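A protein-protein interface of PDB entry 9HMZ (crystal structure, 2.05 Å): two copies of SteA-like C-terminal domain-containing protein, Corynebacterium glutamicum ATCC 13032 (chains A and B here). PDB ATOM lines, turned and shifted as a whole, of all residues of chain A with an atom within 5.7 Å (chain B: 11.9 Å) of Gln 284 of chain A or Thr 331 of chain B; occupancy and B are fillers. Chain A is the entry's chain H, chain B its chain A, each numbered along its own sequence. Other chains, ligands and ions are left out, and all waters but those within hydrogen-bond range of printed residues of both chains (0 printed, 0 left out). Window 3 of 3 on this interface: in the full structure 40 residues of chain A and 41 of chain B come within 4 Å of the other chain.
The side-chain amino group (NZ) of Lys 171 of chain A is in hydrogen-bond range of the backbone carbonyl oxygen (O) of Ser 328 of chain B (3.5 Å).
The backbone carbonyl oxygen of Ser 324 of chain B is in hydrogen-bond range of the side-chain hydroxyl of Ser 328 of chain B (3.0 Å).
O of Arg 170 of chain A sits at hydrogen-bond distance from N of Gln 284 of chain A (2.8 Å).
The side-chain amino group (NZ) of Lys 171 of chain A is in hydrogen-bond range of the side-chain amide oxygen (OE1) of Gln 284 of chain A (2.8 Å).
OD1 of Asn 282 of chain A lies within hydrogen-bond range of NZ of Lys 319 of chain A, 2.8 Å away.
NZ of Lys 319 of chain A is in hydrogen-bond range of O of Pro 283 of chain A.
O of Lys 319 of chain A sits at hydrogen-bond distance from N of Ile 286 of chain A (2.9 Å).
Among the printed residues, pairs that only touch across the chains: Gln 284 of chain A with Ser 328 of chain B (3.5 Å), Gln 284 of chain A with Thr 331 of chain B (3.96 Å), Met 285 of chain A with Val 325 of chain B (3.7 Å) and Lys 319 of chain A with Val 325 of chain B (3.97 Å).
No residue of chain B comes within 4 Å of Gly 169 of chain A.
No residue of chain B comes within 4 Å of Asn 282 of chain A.
Gln 284 of chain A touches two residues of chain B.
Of the printed residues of chain B, Met 285 of chain A touches Val 325.
Phe 191 of chain B touches none of the printed residues of chain A.
Of the printed residues of chain A, Val 325 of chain B touches Met 285 and Lys 319.
Ile 326 of chain B touches none of the printed residues of chain A.
Of the printed residues of chain A, Ser 328 of chain B touches Lys 171 and Gln 284.
Of chain A, only Gln 284 (3.96 Å) comes within 4 Å of Thr 331 of chain B.
The nearest printed residue of chain A that does not touch Val 325 of chain B is Gln 284 of chain A (5.3 Å).
Hydrophobic or aromatic side chains of chain B within 4 Å of the printed part of chain A: Val 325.
Hydrophobic or aromatic side chains of chain A that line the printed part of chain B: Met 285.
Among the printed residues, 5 pairs touch across the chains.
Among the printed residues, no Asp or Glu carboxylate lies within 4 Å of a Lys or Arg side-chain nitrogen of the other chain.
No position is printed for both chains.
Of the 5 pairs that touch across the chains among the printed residues, none has its exchanged pair printed and touching as well.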
ATOM      1  N   ILE A 167      19.225  16.147  21.310  1.00  0.00           N
ATOM      2  CA  ILE A 167      17.884  16.694  21.123  1.00  0.00           C
ATOM      3  C   ILE A 167      17.832  18.222  20.959  1.00  0.00           C
ATOM      4  O   ILE A 167      17.057  18.703  20.137  1.00  0.00           O
ATOM      5  CB  ILE A 167      16.943  16.225  22.266  1.00  0.00           C
ATOM      6  CG1 ILE A 167      16.715  14.705  22.191  1.00  0.00           C
ATOM      7  CG2 ILE A 167      15.604  16.999  22.290  1.00  0.00           C
ATOM      8  CD1 ILE A 167      16.001  14.149  23.350  1.00  0.00           C
ATOM      9  N   GLU A 168      18.607  18.983  21.754  1.00  0.00           N
ATOM     10  CA  GLU A 168      18.544  20.443  21.757  1.00  0.00           C
ATOM     11  C   GLU A 168      18.628  21.081  20.373  1.00  0.00           C
ATOM     12  O   GLU A 168      19.577  20.855  19.638  1.00  0.00           O
ATOM     13  CB  GLU A 168      19.574  21.049  22.714  1.00  0.00           C
ATOM     14  CG  GLU A 168      19.413  22.558  22.858  1.00  0.00           C
ATOM     15  CD  GLU A 168      19.716  23.156  24.220  1.00  0.00           C
ATOM     16  OE1 GLU A 168      20.269  22.433  25.080  1.00  0.00           O
ATOM     17  OE2 GLU A 168      19.396  24.350  24.431  1.00  0.00           O
ATOM     18  N   GLY A 169      17.604  21.850  20.031  1.00  0.00           N
ATOM     19  CA  GLY A 169      17.500  22.550  18.756  1.00  0.00           C
ATOM     20  C   GLY A 169      17.051  21.701  17.576  1.00  0.00           C
ATOM     21  O   GLY A 169      16.858  22.228  16.477  1.00  0.00           O
ATOM     22  N   ARG A 170      16.870  20.387  17.782  1.00  0.00           N
ATOM     23  CA  ARG A 170      16.475  19.495  16.692  1.00  0.00           C
ATOM     24  C   ARG A 170      14.989  19.152  16.693  1.00  0.00           C
ATOM     25  O   ARG A 170      14.320  19.296  17.702  1.00  0.00           O
ATOM     26  CB  ARG A 170      17.306  18.187  16.736  1.00  0.00           C
ATOM     27  CG  ARG A 170      18.812  18.406  16.770  1.00  0.00           C
ATOM     28  CD  ARG A 170      19.535  17.991  15.487  1.00  0.00           C
ATOM     29  NE  ARG A 170      19.040  16.745  14.874  1.00  0.00           N
ATOM     30  CZ  ARG A 170      19.623  15.555  14.994  1.00  0.00           C
ATOM     31  NH1 ARG A 170      20.740  15.423  15.699  1.00  0.00           N
ATOM     32  NH2 ARG A 170      19.090  14.484  14.414  1.00  0.00           N
ATOM     33  N   LYS A 171      14.476  18.692  15.557  1.00  0.00           N
ATOM     34  CA  LYS A 171      13.115  18.178  15.475  1.00  0.00           C
ATOM     35  C   LYS A 171      13.149  16.769  16.081  1.00  0.00           C
ATOM     36  O   LYS A 171      14.111  16.027  15.879  1.00  0.00           O
ATOM     37  CB  LYS A 171      12.642  18.108  14.013  1.00  0.00           C
ATOM     38  CG  LYS A 171      12.546  19.474  13.363  1.00  0.00           C
ATOM     39  CD  LYS A 171      12.089  19.366  11.935  1.00  0.00           C
ATOM     40  CE  LYS A 171      12.034  20.725  11.285  1.00  0.00           C
ATOM     41  NZ  LYS A 171      13.366  21.387  11.294  1.00  0.00           N
ATOM     42  N   ASN A 282      14.903  20.719  25.370  1.00  0.00           N
ATOM     43  CA  ASN A 282      14.713  21.891  24.525  1.00  0.00           C
ATOM     44  C   ASN A 282      14.798  21.609  23.008  1.00  0.00           C
ATOM     45  O   ASN A 282      15.680  22.149  22.324  1.00  0.00           O
ATOM     46  CB  ASN A 282      15.708  22.993  24.954  1.00  0.00           C
ATOM     47  CG  ASN A 282      15.388  24.368  24.440  1.00  0.00           C
ATOM     48  OD1 ASN A 282      14.222  24.712  24.220  1.00  0.00           O
ATOM     49  ND2 ASN A 282      16.413  25.199  24.230  1.00  0.00           N
ATOM     50  N   PRO A 283      13.881  20.790  22.451  1.00  0.00           N
ATOM     51  CA  PRO A 283      13.910  20.555  20.998  1.00  0.00           C
ATOM     52  C   PRO A 283      13.269  21.707  20.210  1.00  0.00           C
ATOM     53  O   PRO A 283      12.665  22.600  20.800  1.00  0.00           O
ATOM     54  CB  PRO A 283      13.080  19.271  20.858  1.00  0.00           C
ATOM     55  CG  PRO A 283      12.089  19.379  21.940  1.00  0.00           C
ATOM     56  CD  PRO A 283      12.731  20.107  23.083  1.00  0.00           C
ATOM     57  N   GLN A 284      13.372  21.683  18.890  1.00  0.00           N
ATOM     58  CA  GLN A 284      12.716  22.683  18.044  1.00  0.00           C
ATOM     59  C   GLN A 284      11.203  22.362  17.994  1.00  0.00           C
ATOM     60  O   GLN A 284      10.369  23.254  18.090  1.00  0.00           O
ATOM     61  CB  GLN A 284      13.327  22.647  16.638  1.00  0.00           C
ATOM     62  CG  GLN A 284      12.776  23.713  15.717  1.00  0.00           C
ATOM     63  CD  GLN A 284      13.468  23.625  14.380  1.00  0.00           C
ATOM     64  OE1 GLN A 284      13.670  22.543  13.843  1.00  0.00           O
ATOM     65  NE2 GLN A 284      13.865  24.768  13.813  1.00  0.00           N
ATOM     66  N   MET A 285      10.862  21.081  17.863  1.00  0.00           N
ATOM     67  CA  MET A 285       9.491  20.600  17.812  1.00  0.00           C
ATOM     68  C   MET A 285       9.453  19.110  18.219  1.00  0.00           C
ATOM     69  O   MET A 285      10.460  18.414  18.134  1.00  0.00           O
ATOM     70  CB  MET A 285       8.918  20.792  16.388  1.00  0.00           C
ATOM     71  CG  MET A 285       9.339  19.682  15.376  1.00  0.00           C
ATOM     72  SD  MET A 285       8.704  20.020  13.728  1.00  0.00           S
ATOM     73  CE  MET A 285       7.382  19.150  13.763  1.00  0.00           C
ATOM     74  N   ILE A 286       8.277  18.623  18.613  1.00  0.00           N
ATOM     75  CA  ILE A 286       8.043  17.243  18.968  1.00  0.00           C
ATOM     76  C   ILE A 286       6.843  16.717  18.167  1.00  0.00           C
ATOM     77  O   ILE A 286       5.719  17.145  18.392  1.00  0.00           O
ATOM     78  CB  ILE A 286       7.817  17.040  20.498  1.00  0.00           C
ATOM     79  CG1 ILE A 286       9.022  17.498  21.314  1.00  0.00           C
ATOM     80  CG2 ILE A 286       7.478  15.569  20.814  1.00  0.00           C
ATOM     81  CD1 ILE A 286       8.698  17.930  22.740  1.00  0.00           C
ATOM     82  N   LYS A 319       5.308  23.361  21.237  1.00  0.00           N
ATOM     83  CA  LYS A 319       6.257  22.468  20.543  1.00  0.00           C
ATOM     84  C   LYS A 319       5.640  21.170  20.032  1.00  0.00           C
ATOM     85  O   LYS A 319       6.204  20.548  19.145  1.00  0.00           O
ATOM     86  CB  LYS A 319       7.465  22.141  21.421  1.00  0.00           C
ATOM     87  CG  LYS A 319       8.339  23.357  21.569  1.00  0.00           C
ATOM     88  CD  LYS A 319       9.639  23.063  22.270  1.00  0.00           C
ATOM     89  CE  LYS A 319      10.434  24.353  22.407  1.00  0.00           C
ATOM     90  NZ  LYS A 319      11.771  24.115  23.008  1.00  0.00           N
ATOM     91  N   SER B 183       5.490  39.226  11.781  1.00  0.00           N
ATOM     92  CA  SER B 183       6.695  38.560  11.302  1.00  0.00           C
ATOM     93  C   SER B 183       6.506  37.034  11.228  1.00  0.00           C
ATOM     94  O   SER B 183       7.161  36.402  10.408  1.00  0.00           O
ATOM     95  CB  SER B 183       7.931  38.977  12.093  1.00  0.00           C
ATOM     96  OG  SER B 183       8.060  38.253  13.304  1.00  0.00           O
ATOM     97  N   ARG B 184       5.589  36.454  12.022  1.00  0.00           N
ATOM     98  CA  ARG B 184       5.289  35.033  11.904  1.00  0.00           C
ATOM     99  C   ARG B 184       4.476  34.794  10.635  1.00  0.00           C
ATOM    100  O   ARG B 184       4.710  33.823   9.933  1.00  0.00           O
ATOM    101  CB  ARG B 184       4.542  34.466  13.116  1.00  0.00           C
ATOM    102  CG  ARG B 184       4.237  32.934  12.929  1.00  0.00           C
ATOM    103  CD  ARG B 184       5.465  32.033  13.071  1.00  0.00           C
ATOM    104  NE  ARG B 184       5.862  31.940  14.480  1.00  0.00           N
ATOM    105  CZ  ARG B 184       7.117  31.948  14.918  1.00  0.00           C
ATOM    106  NH1 ARG B 184       8.125  31.990  14.061  1.00  0.00           N
ATOM    107  NH2 ARG B 184       7.372  31.901  16.220  1.00  0.00           N
ATOM    108  N   LYS B 186       4.638  36.541   7.903  1.00  0.00           N
ATOM    109  CA  LYS B 186       5.590  36.685   6.798  1.00  0.00           C
ATOM    110  C   LYS B 186       6.466  35.436   6.620  1.00  0.00           C
ATOM    111  O   LYS B 186       6.771  35.073   5.494  1.00  0.00           O
ATOM    112  CB  LYS B 186       6.429  37.965   6.937  1.00  0.00           C
ATOM    113  CG  LYS B 186       5.568  39.212   6.817  1.00  0.00           C
ATOM    114  CD  LYS B 186       6.264  40.480   6.368  1.00  0.00           C
ATOM    115  CE  LYS B 186       7.341  40.979   7.290  1.00  0.00           C
ATOM    116  NZ  LYS B 186       7.574  42.439   7.104  1.00  0.00           N
ATOM    117  N   GLU B 187       6.847  34.766   7.711  1.00  0.00           N
ATOM    118  CA  GLU B 187       7.581  33.514   7.642  1.00  0.00           C
ATOM    119  C   GLU B 187       6.720  32.369   7.081  1.00  0.00           C
ATOM    120  O   GLU B 187       7.268  31.346   6.652  1.00  0.00           O
ATOM    121  CB  GLU B 187       8.019  33.073   9.026  1.00  0.00           C
ATOM    122  CG  GLU B 187       8.915  34.025   9.776  1.00  0.00           C
ATOM    123  CD  GLU B 187       9.314  33.475  11.134  1.00  0.00           C
ATOM    124  OE1 GLU B 187       8.564  32.637  11.689  1.00  0.00           O
ATOM    125  OE2 GLU B 187      10.381  33.885  11.647  1.00  0.00           O
ATOM    126  N   LEU B 188       5.394  32.485   7.171  1.00  0.00           N
ATOM    127  CA  LEU B 188       4.466  31.484   6.648  1.00  0.00           C
ATOM    128  C   LEU B 188       3.957  31.821   5.252  1.00  0.00           C
ATOM    129  O   LEU B 188       2.976  31.227   4.826  1.00  0.00           O
ATOM    130  CB  LEU B 188       3.279  31.290   7.585  1.00  0.00           C
ATOM    131  CG  LEU B 188       3.645  30.777   8.957  1.00  0.00           C
ATOM    132  CD1 LEU B 188       2.473  30.902   9.901  1.00  0.00           C
ATOM    133  CD2 LEU B 188       4.203  29.374   8.877  1.00  0.00           C
ATOM    134  N   ARG B 189       4.611  32.755   4.535  1.00  0.00           N
ATOM    135  CA  ARG B 189       4.209  33.120   3.191  1.00  0.00           C
ATOM    136  C   ARG B 189       4.206  31.934   2.231  1.00  0.00           C
ATOM    137  O   ARG B 189       3.241  31.784   1.483  1.00  0.00           O
ATOM    138  CB  ARG B 189       5.100  34.248   2.647  1.00  0.00           C
ATOM    139  CG  ARG B 189       4.673  34.739   1.273  1.00  0.00           C
ATOM    140  CD  ARG B 189       5.409  35.989   0.894  1.00  0.00           C
ATOM    141  NE  ARG B 189       5.040  36.505  -0.422  1.00  0.00           N
ATOM    142  CZ  ARG B 189       4.009  37.320  -0.657  1.00  0.00           C
ATOM    143  NH1 ARG B 189       3.186  37.667   0.333  1.00  0.00           N
ATOM    144  NH2 ARG B 189       3.781  37.776  -1.885  1.00  0.00           N
ATOM    145  N   SER B 190       5.279  31.107   2.230  1.00  0.00           N
ATOM    146  CA  SER B 190       5.341  29.931   1.355  1.00  0.00           C
ATOM    147  C   SER B 190       4.287  28.907   1.729  1.00  0.00           C
ATOM    148  O   SER B 190       3.709  28.302   0.838  1.00  0.00           O
ATOM    149  CB  SER B 190       6.713  29.273   1.405  1.00  0.00           C
ATOM    150  OG  SER B 190       7.690  30.181   0.927  1.00  0.00           O
ATOM    151  N   PHE B 191       4.024  28.716   3.034  1.00  0.00           N
ATOM    152  CA  PHE B 191       2.996  27.796   3.493  1.00  0.00           C
ATOM    153  C   PHE B 191       1.619  28.210   2.960  1.00  0.00           C
ATOM    154  O   PHE B 191       0.892  27.372   2.435  1.00  0.00           O
ATOM    155  CB  PHE B 191       2.970  27.718   5.041  1.00  0.00           C
ATOM    156  CG  PHE B 191       1.811  26.908   5.588  1.00  0.00           C
ATOM    157  CD1 PHE B 191       1.812  25.521   5.510  1.00  0.00           C
ATOM    158  CD2 PHE B 191       0.709  27.535   6.144  1.00  0.00           C
ATOM    159  CE1 PHE B 191       0.736  24.780   5.981  1.00  0.00           C
ATOM    160  CE2 PHE B 191      -0.368  26.796   6.604  1.00  0.00           C
ATOM    161  CZ  PHE B 191      -0.349  25.423   6.522  1.00  0.00           C
ATOM    162  N   GLU B 194       1.466  27.725  -0.905  1.00  0.00           N
ATOM    163  CA  GLU B 194       1.504  26.319  -1.271  1.00  0.00           C
ATOM    164  C   GLU B 194       0.269  25.530  -0.857  1.00  0.00           C
ATOM    165  O   GLU B 194      -0.192  24.669  -1.616  1.00  0.00           O
ATOM    166  CB  GLU B 194       2.783  25.689  -0.701  1.00  0.00           C
ATOM    167  CG  GLU B 194       2.978  24.211  -0.999  1.00  0.00           C
ATOM    168  CD  GLU B 194       4.222  23.596  -0.370  1.00  0.00           C
ATOM    169  OE1 GLU B 194       4.926  24.315   0.383  1.00  0.00           O
ATOM    170  OE2 GLU B 194       4.486  22.393  -0.627  1.00  0.00           O
ATOM    171  N   THR B 294       0.047  28.025  27.213  1.00  0.00           N
ATOM    172  CA  THR B 294       0.722  26.843  27.708  1.00  0.00           C
ATOM    173  C   THR B 294       0.477  26.579  29.210  1.00  0.00           C
ATOM    174  O   THR B 294       0.045  27.481  29.939  1.00  0.00           O
ATOM    175  CB  THR B 294       2.227  26.946  27.386  1.00  0.00           C
ATOM    176  OG1 THR B 294       2.819  27.952  28.217  1.00  0.00           O
ATOM    177  CG2 THR B 294       2.509  27.202  25.904  1.00  0.00           C
ATOM    178  N   VAL B 321      -1.934  23.026  15.652  1.00  0.00           N
ATOM    179  CA  VAL B 321      -0.494  23.146  15.462  1.00  0.00           C
ATOM    180  C   VAL B 321      -0.150  24.645  15.559  1.00  0.00           C
ATOM    181  O   VAL B 321      -0.879  25.480  15.028  1.00  0.00           O
ATOM    182  CB  VAL B 321       0.039  22.473  14.164  1.00  0.00           C
ATOM    183  CG1 VAL B 321      -0.608  23.049  12.917  1.00  0.00           C
ATOM    184  CG2 VAL B 321       1.547  22.578  14.066  1.00  0.00           C
ATOM    185  N   ASP B 322       0.901  24.988  16.310  1.00  0.00           N
ATOM    186  CA  ASP B 322       1.326  26.362  16.438  1.00  0.00           C
ATOM    187  C   ASP B 322       2.013  26.794  15.164  1.00  0.00           C
ATOM    188  O   ASP B 322       2.665  25.978  14.516  1.00  0.00           O
ATOM    189  CB  ASP B 322       2.250  26.562  17.642  1.00  0.00           C
ATOM    190  CG  ASP B 322       2.330  28.038  18.041  1.00  0.00           C
ATOM    191  OD1 ASP B 322       1.330  28.556  18.614  1.00  0.00           O
ATOM    192  OD2 ASP B 322       3.387  28.687  17.752  1.00  0.00           O
ATOM    193  N   GLY B 323       1.888  28.073  14.811  1.00  0.00           N
ATOM    194  CA  GLY B 323       2.509  28.609  13.613  1.00  0.00           C
ATOM    195  C   GLY B 323       4.021  28.456  13.617  1.00  0.00           C
ATOM    196  O   GLY B 323       4.628  28.299  12.558  1.00  0.00           O
ATOM    197  N   SER B 324       4.641  28.447  14.810  1.00  0.00           N
ATOM    198  CA  SER B 324       6.085  28.278  14.932  1.00  0.00           C
ATOM    199  C   SER B 324       6.531  26.874  14.514  1.00  0.00           C
ATOM    200  O   SER B 324       7.640  26.722  13.983  1.00  0.00           O
ATOM    201  CB  SER B 324       6.557  28.592  16.350  1.00  0.00           C
ATOM    202  OG  SER B 324       5.944  27.719  17.277  1.00  0.00           O
ATOM    203  N   VAL B 325       5.682  25.858  14.715  1.00  0.00           N
ATOM    204  CA  VAL B 325       6.012  24.510  14.282  1.00  0.00           C
ATOM    205  C   VAL B 325       6.034  24.462  12.751  1.00  0.00           C
ATOM    206  O   VAL B 325       6.991  23.963  12.164  1.00  0.00           O
ATOM    207  CB  VAL B 325       5.091  23.444  14.912  1.00  0.00           C
ATOM    208  CG1 VAL B 325       5.231  22.096  14.193  1.00  0.00           C
ATOM    209  CG2 VAL B 325       5.388  23.291  16.398  1.00  0.00           C
ATOM    210  N   ILE B 326       5.007  25.023  12.110  1.00  0.00           N
ATOM    211  CA  ILE B 326       4.929  25.083  10.649  1.00  0.00           C
ATOM    212  C   ILE B 326       6.067  25.911  10.061  1.00  0.00           C
ATOM    213  O   ILE B 326       6.668  25.492   9.077  1.00  0.00           O
ATOM    214  CB  ILE B 326       3.558  25.609  10.190  1.00  0.00           C
ATOM    215  CG1 ILE B 326       2.408  24.747  10.747  1.00  0.00           C
ATOM    216  CG2 ILE B 326       3.498  25.691   8.693  1.00  0.00           C
ATOM    217  CD1 ILE B 326       2.432  23.265  10.314  1.00  0.00           C
ATOM    218  N   ALA B 327       6.410  27.056  10.676  1.00  0.00           N
ATOM    219  CA  ALA B 327       7.501  27.912  10.183  1.00  0.00           C
ATOM    220  C   ALA B 327       8.860  27.211  10.253  1.00  0.00           C
ATOM    221  O   ALA B 327       9.694  27.427   9.373  1.00  0.00           O
ATOM    222  CB  ALA B 327       7.533  29.241  10.934  1.00  0.00           C
ATOM    223  N   SER B 328       9.075  26.340  11.262  1.00  0.00           N
ATOM    224  CA  SER B 328      10.305  25.531  11.399  1.00  0.00           C
ATOM    225  C   SER B 328      10.509  24.551  10.240  1.00  0.00           C
ATOM    226  O   SER B 328      11.633  24.090  10.014  1.00  0.00           O
ATOM    227  CB  SER B 328      10.301  24.755  12.712  1.00  0.00           C
ATOM    228  OG  SER B 328      10.461  25.648  13.802  1.00  0.00           O
ATOM    229  N   LEU B 329       9.436  24.202   9.513  1.00  0.00           N
ATOM    230  CA  LEU B 329       9.557  23.330   8.348  1.00  0.00           C
ATOM    231  C   LEU B 329      10.175  24.064   7.130  1.00  0.00           C
ATOM    232  O   LEU B 329      10.627  23.408   6.186  1.00  0.00           O
ATOM    233  CB  LEU B 329       8.193  22.743   7.986  1.00  0.00           C
ATOM    234  CG  LEU B 329       7.534  21.922   9.100  1.00  0.00           C
ATOM    235  CD1 LEU B 329       6.136  21.542   8.730  1.00  0.00           C
ATOM    236  CD2 LEU B 329       8.361  20.685   9.458  1.00  0.00           C
ATOM    237  N   TYR B 330      10.217  25.408   7.167  1.00  0.00           N
ATOM    238  CA  TYR B 330      10.737  26.262   6.110  1.00  0.00           C
ATOM    239  C   TYR B 330      12.110  26.866   6.414  1.00  0.00           C
ATOM    240  O   TYR B 330      12.768  27.338   5.492  1.00  0.00           O
ATOM    241  CB  TYR B 330       9.718  27.359   5.775  1.00  0.00           C
ATOM    242  CG  TYR B 330       8.470  26.789   5.141  1.00  0.00           C
ATOM    243  CD1 TYR B 330       8.412  26.546   3.780  1.00  0.00           C
ATOM    244  CD2 TYR B 330       7.384  26.406   5.917  1.00  0.00           C
ATOM    245  CE1 TYR B 330       7.287  25.992   3.194  1.00  0.00           C
ATOM    246  CE2 TYR B 330       6.259  25.821   5.346  1.00  0.00           C
ATOM    247  CZ  TYR B 330       6.211  25.626   3.977  1.00  0.00           C
ATOM    248  OH  TYR B 330       5.113  25.054   3.384  1.00  0.00           O
ATOM    249  N   THR B 331      12.559  26.824   7.680  1.00  0.00           N
ATOM    250  CA  THR B 331      13.857  27.355   8.101  1.00  0.00           C
ATOM    251  C   THR B 331      15.030  26.704   7.352  1.00  0.00           C
ATOM    252  O   THR B 331      15.059  25.479   7.178  1.00  0.00           O
ATOM    253  CB  THR B 331      14.028  27.219   9.626  1.00  0.00           C
ATOM    254  OG1 THR B 331      13.967  25.835  10.004  1.00  0.00           O
ATOM    255  CG2 THR B 331      13.007  28.040  10.409  1.00  0.00           C
